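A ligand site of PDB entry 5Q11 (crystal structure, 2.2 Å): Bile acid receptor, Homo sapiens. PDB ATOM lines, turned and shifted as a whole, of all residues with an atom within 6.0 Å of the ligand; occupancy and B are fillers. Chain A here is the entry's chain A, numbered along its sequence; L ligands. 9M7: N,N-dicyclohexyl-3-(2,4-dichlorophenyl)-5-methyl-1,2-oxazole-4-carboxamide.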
ATOM      1  N   PHE A  45      -8.296  11.033  33.973  1.00  0.00           N
ATOM      2  CA  PHE A  45      -7.183  11.054  33.033  1.00  0.00           C
ATOM      3  C   PHE A  45      -7.688  10.757  31.600  1.00  0.00           C
ATOM      4  O   PHE A  45      -7.205  11.374  30.650  1.00  0.00           O
ATOM      5  CB  PHE A  45      -6.054  10.090  33.447  1.00  0.00           C
ATOM      6  CG  PHE A  45      -4.785  10.267  32.663  1.00  0.00           C
ATOM      7  CD1 PHE A  45      -4.560   9.536  31.500  1.00  0.00           C
ATOM      8  CD2 PHE A  45      -3.828  11.196  33.056  1.00  0.00           C
ATOM      9  CE1 PHE A  45      -3.393   9.719  30.754  1.00  0.00           C
ATOM     10  CE2 PHE A  45      -2.656  11.380  32.319  1.00  0.00           C
ATOM     11  CZ  PHE A  45      -2.435  10.631  31.173  1.00  0.00           C
ATOM     12  N   LEU A  48      -9.384  13.938  30.071  1.00  0.00           N
ATOM     13  CA  LEU A  48      -8.352  14.900  29.684  1.00  0.00           C
ATOM     14  C   LEU A  48      -7.704  14.468  28.379  1.00  0.00           C
ATOM     15  O   LEU A  48      -7.464  15.317  27.524  1.00  0.00           O
ATOM     16  CB  LEU A  48      -7.291  15.051  30.797  1.00  0.00           C
ATOM     17  CG  LEU A  48      -7.795  15.501  32.166  1.00  0.00           C
ATOM     18  CD1 LEU A  48      -6.692  15.461  33.195  1.00  0.00           C
ATOM     19  CD2 LEU A  48      -8.416  16.884  32.109  1.00  0.00           C
ATOM     20  N   THR A  49      -7.473  13.150  28.219  1.00  0.00           N
ATOM     21  CA  THR A  49      -6.902  12.555  27.005  1.00  0.00           C
ATOM     22  C   THR A  49      -7.815  12.857  25.802  1.00  0.00           C
ATOM     23  O   THR A  49      -7.309  13.222  24.741  1.00  0.00           O
ATOM     24  CB  THR A  49      -6.649  11.062  27.207  1.00  0.00           C
ATOM     25  OG1 THR A  49      -5.840  10.887  28.362  1.00  0.00           O
ATOM     26  CG2 THR A  49      -5.936  10.430  26.041  1.00  0.00           C
ATOM     27  N   MET A  51     -10.096  15.439  25.613  1.00  0.00           N
ATOM     28  CA  MET A  51     -10.041  16.886  25.430  1.00  0.00           C
ATOM     29  C   MET A  51      -8.782  17.245  24.688  1.00  0.00           C
ATOM     30  O   MET A  51      -8.861  18.041  23.763  1.00  0.00           O
ATOM     31  CB  MET A  51     -10.073  17.617  26.770  1.00  0.00           C
ATOM     32  CG  MET A  51     -11.425  17.597  27.407  1.00  0.00           C
ATOM     33  SD  MET A  51     -11.370  18.278  29.065  1.00  0.00           S
ATOM     34  CE  MET A  51     -11.508  20.004  28.693  1.00  0.00           C
ATOM     35  N   ALA A  52      -7.642  16.598  25.042  1.00  0.00           N
ATOM     36  CA  ALA A  52      -6.323  16.817  24.411  1.00  0.00           C
ATOM     37  C   ALA A  52      -6.340  16.481  22.921  1.00  0.00           C
ATOM     38  O   ALA A  52      -5.890  17.282  22.121  1.00  0.00           O
ATOM     39  CB  ALA A  52      -5.229  16.017  25.131  1.00  0.00           C
ATOM     40  N   THR A  53      -6.929  15.342  22.554  1.00  0.00           N
ATOM     41  CA  THR A  53      -7.088  14.851  21.171  1.00  0.00           C
ATOM     42  C   THR A  53      -7.934  15.813  20.362  1.00  0.00           C
ATOM     43  O   THR A  53      -7.582  16.131  19.235  1.00  0.00           O
ATOM     44  CB  THR A  53      -7.693  13.437  21.214  1.00  0.00           C
ATOM     45  OG1 THR A  53      -6.897  12.651  22.102  1.00  0.00           O
ATOM     46  CG2 THR A  53      -7.734  12.778  19.839  1.00  0.00           C
ATOM     47  N   HIS A  55      -8.423  19.088  21.101  1.00  0.00           N
ATOM     48  CA  HIS A  55      -7.663  20.339  20.961  1.00  0.00           C
ATOM     49  C   HIS A  55      -6.749  20.262  19.742  1.00  0.00           C
ATOM     50  O   HIS A  55      -6.745  21.164  18.918  1.00  0.00           O
ATOM     51  CB  HIS A  55      -6.853  20.681  22.238  1.00  0.00           C
ATOM     52  CG  HIS A  55      -7.683  21.047  23.438  1.00  0.00           C
ATOM     53  ND1 HIS A  55      -7.124  21.072  24.708  1.00  0.00           N
ATOM     54  CD2 HIS A  55      -8.985  21.381  23.529  1.00  0.00           C
ATOM     55  CE1 HIS A  55      -8.098  21.426  25.528  1.00  0.00           C
ATOM     56  NE2 HIS A  55      -9.244  21.622  24.869  1.00  0.00           N
ATOM     57  N   ALA A  85       2.635  22.224  19.454  1.00  0.00           N
ATOM     58  CA  ALA A  85       1.518  21.470  20.019  1.00  0.00           C
ATOM     59  C   ALA A  85       1.181  21.810  21.464  1.00  0.00           C
ATOM     60  O   ALA A  85       0.105  22.345  21.733  1.00  0.00           O
ATOM     61  CB  ALA A  85       1.778  19.980  19.874  1.00  0.00           C
ATOM     62  N   VAL A  86       2.101  21.485  22.394  1.00  0.00           N
ATOM     63  CA  VAL A  86       1.971  21.683  23.838  1.00  0.00           C
ATOM     64  C   VAL A  86       1.611  23.134  24.142  1.00  0.00           C
ATOM     65  O   VAL A  86       0.635  23.371  24.848  1.00  0.00           O
ATOM     66  CB  VAL A  86       3.273  21.232  24.575  1.00  0.00           C
ATOM     67  CG1 VAL A  86       3.249  21.604  26.061  1.00  0.00           C
ATOM     68  CG2 VAL A  86       3.536  19.740  24.393  1.00  0.00           C
ATOM     69  N   GLU A  87       2.373  24.089  23.580  1.00  0.00           N
ATOM     70  CA  GLU A  87       2.176  25.515  23.753  1.00  0.00           C
ATOM     71  C   GLU A  87       0.786  25.985  23.267  1.00  0.00           C
ATOM     72  O   GLU A  87       0.072  26.664  24.016  1.00  0.00           O
ATOM     73  CB  GLU A  87       3.293  26.276  23.034  1.00  0.00           C
ATOM     74  CG  GLU A  87       4.600  26.350  23.807  1.00  0.00           C
ATOM     75  CD  GLU A  87       5.759  26.921  23.004  1.00  0.00           C
ATOM     76  OE1 GLU A  87       5.601  27.996  22.374  1.00  0.00           O
ATOM     77  OE2 GLU A  87       6.833  26.287  22.997  1.00  0.00           O
ATOM     78  N   MET A  89      -1.897  24.143  22.770  1.00  0.00           N
ATOM     79  CA  MET A  89      -2.913  23.442  23.572  1.00  0.00           C
ATOM     80  C   MET A  89      -3.158  24.146  24.880  1.00  0.00           C
ATOM     81  O   MET A  89      -4.330  24.352  25.214  1.00  0.00           O
ATOM     82  CB  MET A  89      -2.554  21.985  23.822  1.00  0.00           C
ATOM     83  CG  MET A  89      -2.706  21.133  22.599  1.00  0.00           C
ATOM     84  SD  MET A  89      -1.836  19.567  22.799  1.00  0.00           S
ATOM     85  CE  MET A  89      -3.010  18.691  23.885  1.00  0.00           C
ATOM     86  N   PHE A  90      -2.090  24.528  25.606  1.00  0.00           N
ATOM     87  CA  PHE A  90      -2.251  25.250  26.872  1.00  0.00           C
ATOM     88  C   PHE A  90      -2.957  26.576  26.696  1.00  0.00           C
ATOM     89  O   PHE A  90      -3.821  26.912  27.498  1.00  0.00           O
ATOM     90  CB  PHE A  90      -0.934  25.420  27.650  1.00  0.00           C
ATOM     91  CG  PHE A  90      -0.621  24.203  28.486  1.00  0.00           C
ATOM     92  CD1 PHE A  90      -1.445  23.830  29.542  1.00  0.00           C
ATOM     93  CD2 PHE A  90       0.486  23.413  28.196  1.00  0.00           C
ATOM     94  CE1 PHE A  90      -1.200  22.657  30.261  1.00  0.00           C
ATOM     95  CE2 PHE A  90       0.767  22.273  28.959  1.00  0.00           C
ATOM     96  CZ  PHE A  90      -0.083  21.895  29.973  1.00  0.00           C
ATOM     97  N   LEU A  91      -2.614  27.297  25.606  1.00  0.00           N
ATOM     98  CA  LEU A  91      -3.235  28.555  25.247  1.00  0.00           C
ATOM     99  C   LEU A  91      -4.745  28.373  25.000  1.00  0.00           C
ATOM    100  O   LEU A  91      -5.550  29.166  25.507  1.00  0.00           O
ATOM    101  CB  LEU A  91      -2.520  29.167  24.026  1.00  0.00           C
ATOM    102  CG  LEU A  91      -2.634  30.677  23.820  1.00  0.00           C
ATOM    103  CD1 LEU A  91      -2.443  31.453  25.124  1.00  0.00           C
ATOM    104  CD2 LEU A  91      -1.620  31.156  22.800  1.00  0.00           C
ATOM    105  N   SER A  93      -6.584  25.717  26.130  1.00  0.00           N
ATOM    106  CA  SER A  93      -7.192  25.239  27.374  1.00  0.00           C
ATOM    107  C   SER A  93      -7.412  26.374  28.375  1.00  0.00           C
ATOM    108  O   SER A  93      -8.427  26.363  29.065  1.00  0.00           O
ATOM    109  CB  SER A  93      -6.391  24.087  27.975  1.00  0.00           C
ATOM    110  OG  SER A  93      -5.124  24.536  28.430  1.00  0.00           O
ATOM    111  N   PHE A  97     -10.954  27.291  29.886  1.00  0.00           N
ATOM    112  CA  PHE A  97     -11.074  27.377  31.337  1.00  0.00           C
ATOM    113  C   PHE A  97     -11.557  28.745  31.845  1.00  0.00           C
ATOM    114  O   PHE A  97     -12.492  28.790  32.644  1.00  0.00           O
ATOM    115  CB  PHE A  97      -9.774  26.958  32.024  1.00  0.00           C
ATOM    116  CG  PHE A  97      -9.919  26.647  33.495  1.00  0.00           C
ATOM    117  CD1 PHE A  97     -10.334  25.387  33.921  1.00  0.00           C
ATOM    118  CD2 PHE A  97      -9.633  27.611  34.458  1.00  0.00           C
ATOM    119  CE1 PHE A  97     -10.464  25.106  35.284  1.00  0.00           C
ATOM    120  CE2 PHE A  97      -9.758  27.322  35.820  1.00  0.00           C
ATOM    121  CZ  PHE A  97     -10.191  26.080  36.218  1.00  0.00           C
ATOM    122  N   LEU A 109     -13.992  20.632  36.391  1.00  0.00           N
ATOM    123  CA  LEU A 109     -12.822  20.325  35.577  1.00  0.00           C
ATOM    124  C   LEU A 109     -11.522  20.384  36.403  1.00  0.00           C
ATOM    125  O   LEU A 109     -10.684  19.489  36.266  1.00  0.00           O
ATOM    126  CB  LEU A 109     -12.757  21.235  34.349  1.00  0.00           C
ATOM    127  CG  LEU A 109     -11.652  20.908  33.341  1.00  0.00           C
ATOM    128  CD1 LEU A 109     -11.680  19.405  32.949  1.00  0.00           C
ATOM    129  CD2 LEU A 109     -11.719  21.857  32.141  1.00  0.00           C
ATOM    130  N   ILE A 113      -8.848  17.455  37.022  1.00  0.00           N
ATOM    131  CA  ILE A 113      -7.439  17.699  36.744  1.00  0.00           C
ATOM    132  C   ILE A 113      -6.585  17.329  37.956  1.00  0.00           C
ATOM    133  O   ILE A 113      -5.666  16.533  37.828  1.00  0.00           O
ATOM    134  CB  ILE A 113      -7.197  19.165  36.268  1.00  0.00           C
ATOM    135  CG1 ILE A 113      -7.757  19.390  34.838  1.00  0.00           C
ATOM    136  CG2 ILE A 113      -5.697  19.547  36.354  1.00  0.00           C
ATOM    137  CD1 ILE A 113      -7.999  20.876  34.465  1.00  0.00           C
ATOM    138  N   ILE A 118      -1.807  13.204  37.505  1.00  0.00           N
ATOM    139  CA  ILE A 118      -0.813  14.170  37.047  1.00  0.00           C
ATOM    140  C   ILE A 118      -0.256  14.887  38.301  1.00  0.00           C
ATOM    141  O   ILE A 118      -1.025  15.194  39.212  1.00  0.00           O
ATOM    142  CB  ILE A 118      -1.441  15.116  35.977  1.00  0.00           C
ATOM    143  CG1 ILE A 118      -1.982  14.279  34.789  1.00  0.00           C
ATOM    144  CG2 ILE A 118      -0.439  16.175  35.480  1.00  0.00           C
ATOM    145  CD1 ILE A 118      -2.983  14.949  33.876  1.00  0.00           C
ATOM    146  N   TYR A 122       3.224  19.946  37.831  1.00  0.00           N
ATOM    147  CA  TYR A 122       2.732  20.292  36.496  1.00  0.00           C
ATOM    148  C   TYR A 122       1.478  21.160  36.631  1.00  0.00           C
ATOM    149  O   TYR A 122       1.375  22.219  36.005  1.00  0.00           O
ATOM    150  CB  TYR A 122       2.403  19.004  35.719  1.00  0.00           C
ATOM    151  CG  TYR A 122       2.291  19.116  34.206  1.00  0.00           C
ATOM    152  CD1 TYR A 122       2.119  20.357  33.576  1.00  0.00           C
ATOM    153  CD2 TYR A 122       2.320  17.981  33.391  1.00  0.00           C
ATOM    154  CE1 TYR A 122       2.021  20.462  32.196  1.00  0.00           C
ATOM    155  CE2 TYR A 122       2.203  18.075  32.014  1.00  0.00           C
ATOM    156  CZ  TYR A 122       2.051  19.320  31.417  1.00  0.00           C
ATOM    157  OH  TYR A 122       1.947  19.431  30.053  1.00  0.00           O
ATOM    158  N   ILE A 123       0.510  20.690  37.445  1.00  0.00           N
ATOM    159  CA  ILE A 123      -0.805  21.296  37.639  1.00  0.00           C
ATOM    160  C   ILE A 123      -0.749  22.713  38.248  1.00  0.00           C
ATOM    161  O   ILE A 123      -1.538  23.559  37.831  1.00  0.00           O
ATOM    162  CB  ILE A 123      -1.692  20.315  38.457  1.00  0.00           C
ATOM    163  CG1 ILE A 123      -2.074  19.084  37.599  1.00  0.00           C
ATOM    164  CG2 ILE A 123      -2.939  20.983  39.049  1.00  0.00           C
ATOM    165  CD1 ILE A 123      -2.662  17.890  38.381  1.00  0.00           C
ATOM    166  N   MET A 126       0.350  25.428  35.689  1.00  0.00           N
ATOM    167  CA  MET A 126      -0.730  25.459  34.705  1.00  0.00           C
ATOM    168  C   MET A 126      -1.821  26.420  35.164  1.00  0.00           C
ATOM    169  O   MET A 126      -2.229  27.277  34.385  1.00  0.00           O
ATOM    170  CB  MET A 126      -1.317  24.054  34.465  1.00  0.00           C
ATOM    171  CG  MET A 126      -2.342  24.050  33.346  1.00  0.00           C
ATOM    172  SD  MET A 126      -3.529  22.707  33.322  1.00  0.00           S
ATOM    173  CE  MET A 126      -4.505  23.129  34.605  1.00  0.00           C
ATOM    174  N   TYR A 130      -3.020  30.046  33.900  1.00  0.00           N
ATOM    175  CA  TYR A 130      -4.435  30.311  33.621  1.00  0.00           C
ATOM    176  C   TYR A 130      -4.895  31.593  34.278  1.00  0.00           C
ATOM    177  O   TYR A 130      -5.600  32.378  33.642  1.00  0.00           O
ATOM    178  CB  TYR A 130      -5.334  29.158  34.115  1.00  0.00           C
ATOM    179  CG  TYR A 130      -5.398  27.909  33.277  1.00  0.00           C
ATOM    180  CD1 TYR A 130      -4.595  27.743  32.150  1.00  0.00           C
ATOM    181  CD2 TYR A 130      -6.258  26.862  33.629  1.00  0.00           C
ATOM    182  CE1 TYR A 130      -4.647  26.577  31.389  1.00  0.00           C
ATOM    183  CE2 TYR A 130      -6.337  25.706  32.859  1.00  0.00           C
ATOM    184  CZ  TYR A 130      -5.519  25.569  31.742  1.00  0.00           C
ATOM    185  OH  TYR A 130      -5.567  24.394  31.038  1.00  0.00           O
ATOM    186  N   HIS A 208       5.833  19.093  30.556  1.00  0.00           N
ATOM    187  CA  HIS A 208       5.201  18.028  29.758  1.00  0.00           C
ATOM    188  C   HIS A 208       6.193  16.915  29.450  1.00  0.00           C
ATOM    189  O   HIS A 208       5.813  15.735  29.443  1.00  0.00           O
ATOM    190  CB  HIS A 208       4.619  18.587  28.439  1.00  0.00           C
ATOM    191  CG  HIS A 208       3.729  17.636  27.701  1.00  0.00           C
ATOM    192  ND1 HIS A 208       2.411  17.444  28.081  1.00  0.00           N
ATOM    193  CD2 HIS A 208       3.986  16.859  26.620  1.00  0.00           C
ATOM    194  CE1 HIS A 208       1.917  16.551  27.247  1.00  0.00           C
ATOM    195  NE2 HIS A 208       2.835  16.160  26.350  1.00  0.00           N
ATOM    196  N   MET A 211       6.668  14.793  32.447  1.00  0.00           N
ATOM    197  CA  MET A 211       5.454  14.029  32.683  1.00  0.00           C
ATOM    198  C   MET A 211       5.449  12.777  31.786  1.00  0.00           C
ATOM    199  O   MET A 211       5.171  11.678  32.285  1.00  0.00           O
ATOM    200  CB  MET A 211       4.194  14.876  32.447  1.00  0.00           C
ATOM    201  CG  MET A 211       2.903  14.149  32.749  1.00  0.00           C
ATOM    202  SD  MET A 211       1.669  14.359  31.436  1.00  0.00           S
ATOM    203  CE  MET A 211       2.266  13.204  30.219  1.00  0.00           C
ATOM    204  N   PHE A 222      -2.288   6.990  25.825  1.00  0.00           N
ATOM    205  CA  PHE A 222      -2.896   8.168  25.209  1.00  0.00           C
ATOM    206  C   PHE A 222      -3.709   7.787  23.950  1.00  0.00           C
ATOM    207  O   PHE A 222      -4.471   6.827  24.007  1.00  0.00           O
ATOM    208  CB  PHE A 222      -1.820   9.239  24.911  1.00  0.00           C
ATOM    209  CG  PHE A 222      -0.784   9.395  25.991  1.00  0.00           C
ATOM    210  CD1 PHE A 222      -1.066  10.082  27.170  1.00  0.00           C
ATOM    211  CD2 PHE A 222       0.492   8.865  25.835  1.00  0.00           C
ATOM    212  CE1 PHE A 222      -0.106  10.225  28.169  1.00  0.00           C
ATOM    213  CE2 PHE A 222       1.455   8.995  26.846  1.00  0.00           C
ATOM    214  CZ  PHE A 222       1.153   9.687  28.001  1.00  0.00           C
ATOM    215  N   LEU A 226      -2.082  11.961  19.799  1.00  0.00           N
ATOM    216  CA  LEU A 226      -1.272  12.449  20.916  1.00  0.00           C
ATOM    217  C   LEU A 226       0.156  11.874  20.874  1.00  0.00           C
ATOM    218  O   LEU A 226       1.096  12.638  21.063  1.00  0.00           O
ATOM    219  CB  LEU A 226      -1.940  12.180  22.276  1.00  0.00           C
ATOM    220  CG  LEU A 226      -3.181  13.006  22.608  1.00  0.00           C
ATOM    221  CD1 LEU A 226      -3.634  12.725  24.027  1.00  0.00           C
ATOM    222  CD2 LEU A 226      -2.953  14.516  22.394  1.00  0.00           C
ATOM    223  N   TRP A 230       3.167  14.424  20.068  1.00  0.00           N
ATOM    224  CA  TRP A 230       4.071  14.531  21.212  1.00  0.00           C
ATOM    225  C   TRP A 230       5.232  13.565  21.029  1.00  0.00           C
ATOM    226  O   TRP A 230       6.210  13.619  21.769  1.00  0.00           O
ATOM    227  CB  TRP A 230       3.348  14.238  22.549  1.00  0.00           C
ATOM    228  CG  TRP A 230       2.243  15.180  22.949  1.00  0.00           C
ATOM    229  CD1 TRP A 230       2.115  16.506  22.645  1.00  0.00           C
ATOM    230  CD2 TRP A 230       1.180  14.889  23.881  1.00  0.00           C
ATOM    231  NE1 TRP A 230       1.023  17.048  23.300  1.00  0.00           N
ATOM    232  CE2 TRP A 230       0.443  16.070  24.061  1.00  0.00           C
ATOM    233  CE3 TRP A 230       0.811  13.733  24.595  1.00  0.00           C
ATOM    234  CZ2 TRP A 230      -0.682  16.132  24.903  1.00  0.00           C
ATOM    235  CZ3 TRP A 230      -0.302  13.791  25.430  1.00  0.00           C
ATOM    236  CH2 TRP A 230      -1.040  14.979  25.575  1.00  0.00           C
HETATM  237  N1  9M7 L   1      -2.753  17.619  29.484  1.00  0.00           N
HETATM  238  C4  9M7 L   1      -2.795  16.137  29.652  1.00  0.00           C
HETATM  239  C5  9M7 L   1      -2.668  19.584  27.862  1.00  0.00           C
HETATM  240  C7  9M7 L   1      -1.440  18.355  31.523  1.00  0.00           C
HETATM  241  C8  9M7 L   1      -4.000  18.240  31.590  1.00  0.00           C
HETATM  242  C10 9M7 L   1      -1.459  15.472  29.230  1.00  0.00           C
HETATM  243  C13 9M7 L   1      -1.461  19.342  32.706  1.00  0.00           C
HETATM  244  C15 9M7 L   1      -4.006  13.943  29.210  1.00  0.00           C
HETATM  245  C17 9M7 L   1      -4.954  20.499  28.878  1.00  0.00           C
HETATM  246  C20 9M7 L   1      -0.394  19.876  26.593  1.00  0.00           C
HETATM  247  C21 9M7 L   1      -2.674  19.115  33.603  1.00  0.00           C
HETATM  248  C22 9M7 L   1      -2.702  13.323  28.707  1.00  0.00           C
HETATM  249  C24 9M7 L   1      -5.180  21.334  29.980  1.00  0.00           C
HETATM  250  C28 9M7 L   1      -7.353  20.416  30.267  1.00  0.00           C
HETATM  251  C12 9M7 L   1      -1.686  20.274  27.199  1.00  0.00           C
HETATM  252  O19 9M7 L   1      -2.036  21.567  27.105  1.00  0.00           O
HETATM  253  N18 9M7 L   1      -3.292  21.763  27.728  1.00  0.00           N
HETATM  254  C11 9M7 L   1      -3.661  20.580  28.175  1.00  0.00           C
HETATM  255  C27 9M7 L   1      -6.375  21.297  30.666  1.00  0.00           C
HETATM  256 CL29 9M7 L   1      -8.846  20.358  31.125  1.00  0.00          CL
HETATM  257  C25 9M7 L   1      -7.185  19.568  29.190  1.00  0.00           C
HETATM  258  C23 9M7 L   1      -5.987  19.619  28.501  1.00  0.00           C
HETATM  259 CL26 9M7 L   1      -5.817  18.545  27.168  1.00  0.00          CL
HETATM  260  C2  9M7 L   1      -2.714  18.113  28.196  1.00  0.00           C
HETATM  261  O6  9M7 L   1      -2.706  17.372  27.190  1.00  0.00           O
HETATM  262  C3  9M7 L   1      -2.753  18.435  30.711  1.00  0.00           C
HETATM  263  C14 9M7 L   1      -3.995  19.216  32.781  1.00  0.00           C
HETATM  264  C9  9M7 L   1      -4.024  15.461  28.991  1.00  0.00           C
HETATM  265  C16 9M7 L   1      -1.499  13.941  29.415  1.00  0.00           C
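O19 of the ligand sits close to N of Phe 90 (3.3 Å). The side-chain hydroxyl of Ser 93 lies within hydrogen-bond range of a nitrogen (N18) of the ligand, 3.4 Å away.
Phe 45 touches the ligand. Leu 48 touches the ligand (CD2 to CL29, 3.6 Å). Thr 49 touches the ligand. CE of Met 51 touches CL29 of the ligand, 3.6 Å away. CA of Ala 52 touches CL26 of the ligand, at 3.3 Å. ND1 of His 55 touches CL26 of the ligand, 3.8 Å away. Val 86 touches the ligand. CB of Met 89 touches O19 of the ligand, at 3.3 Å. Leu 109 touches the ligand. Ile 113 touches the ligand (CD1 to CL29, 3.5 Å). Tyr 122 touches the ligand. SD of Met 126 touches C14 of the ligand, 3.6 Å away. OH of Tyr 130 touches C27 of the ligand, at 3.2 Å. ND1 of His 208 touches C20 of the ligand, 3.9996 Å away. Met 211 touches the ligand. Phe 222 touches the ligand (CD1 to C22, 3.9 Å). Trp 230 touches the ligand (CZ2 to O6, 3.3 Å). Hydrophobic or aromatic side chains that line the ligand: Phe 45, Leu 48, Met 51, Ala 52, Met 89, Phe 90, Leu 109, Ile 113, Tyr 122, Met 126, Met 211, Phe 222 and Trp 230. Of the 27 residues printed, 19 come within 4 Å of the ligand. The nearest printed residue that does not touch the ligand is Ile 123 (4.04 Å).
OH of Tyr 130 is in hydrogen-bond range of OG of Ser 93 (2.6 Å). The side-chain hydroxyl (OH) of Tyr 130 lies within hydrogen-bond range of the side-chain sulfur (SD) of Met 126. O of Phe 90 lies within hydrogen-bond range of OG of Ser 93 (2.9 Å). The backbone carbonyl oxygen (O) of Met 89 lies within hydrogen-bond range of the side-chain hydroxyl (OG) of Ser 93, 3.3 Å away. A ring nitrogen (ND1) of His 208 is in hydrogen-bond range of the side-chain hydroxyl (OH) of Tyr 122, 2.8 Å away. The backbone carbonyl oxygen (O) of Phe 45 is in hydrogen-bond range of the side-chain hydroxyl (OG1) of Thr 49, at 2.7 Å. The backbone carbonyl oxygen (O) of Thr 49 lies within hydrogen-bond range of the side-chain hydroxyl (OG1) of Thr 53, 2.7 Å away.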
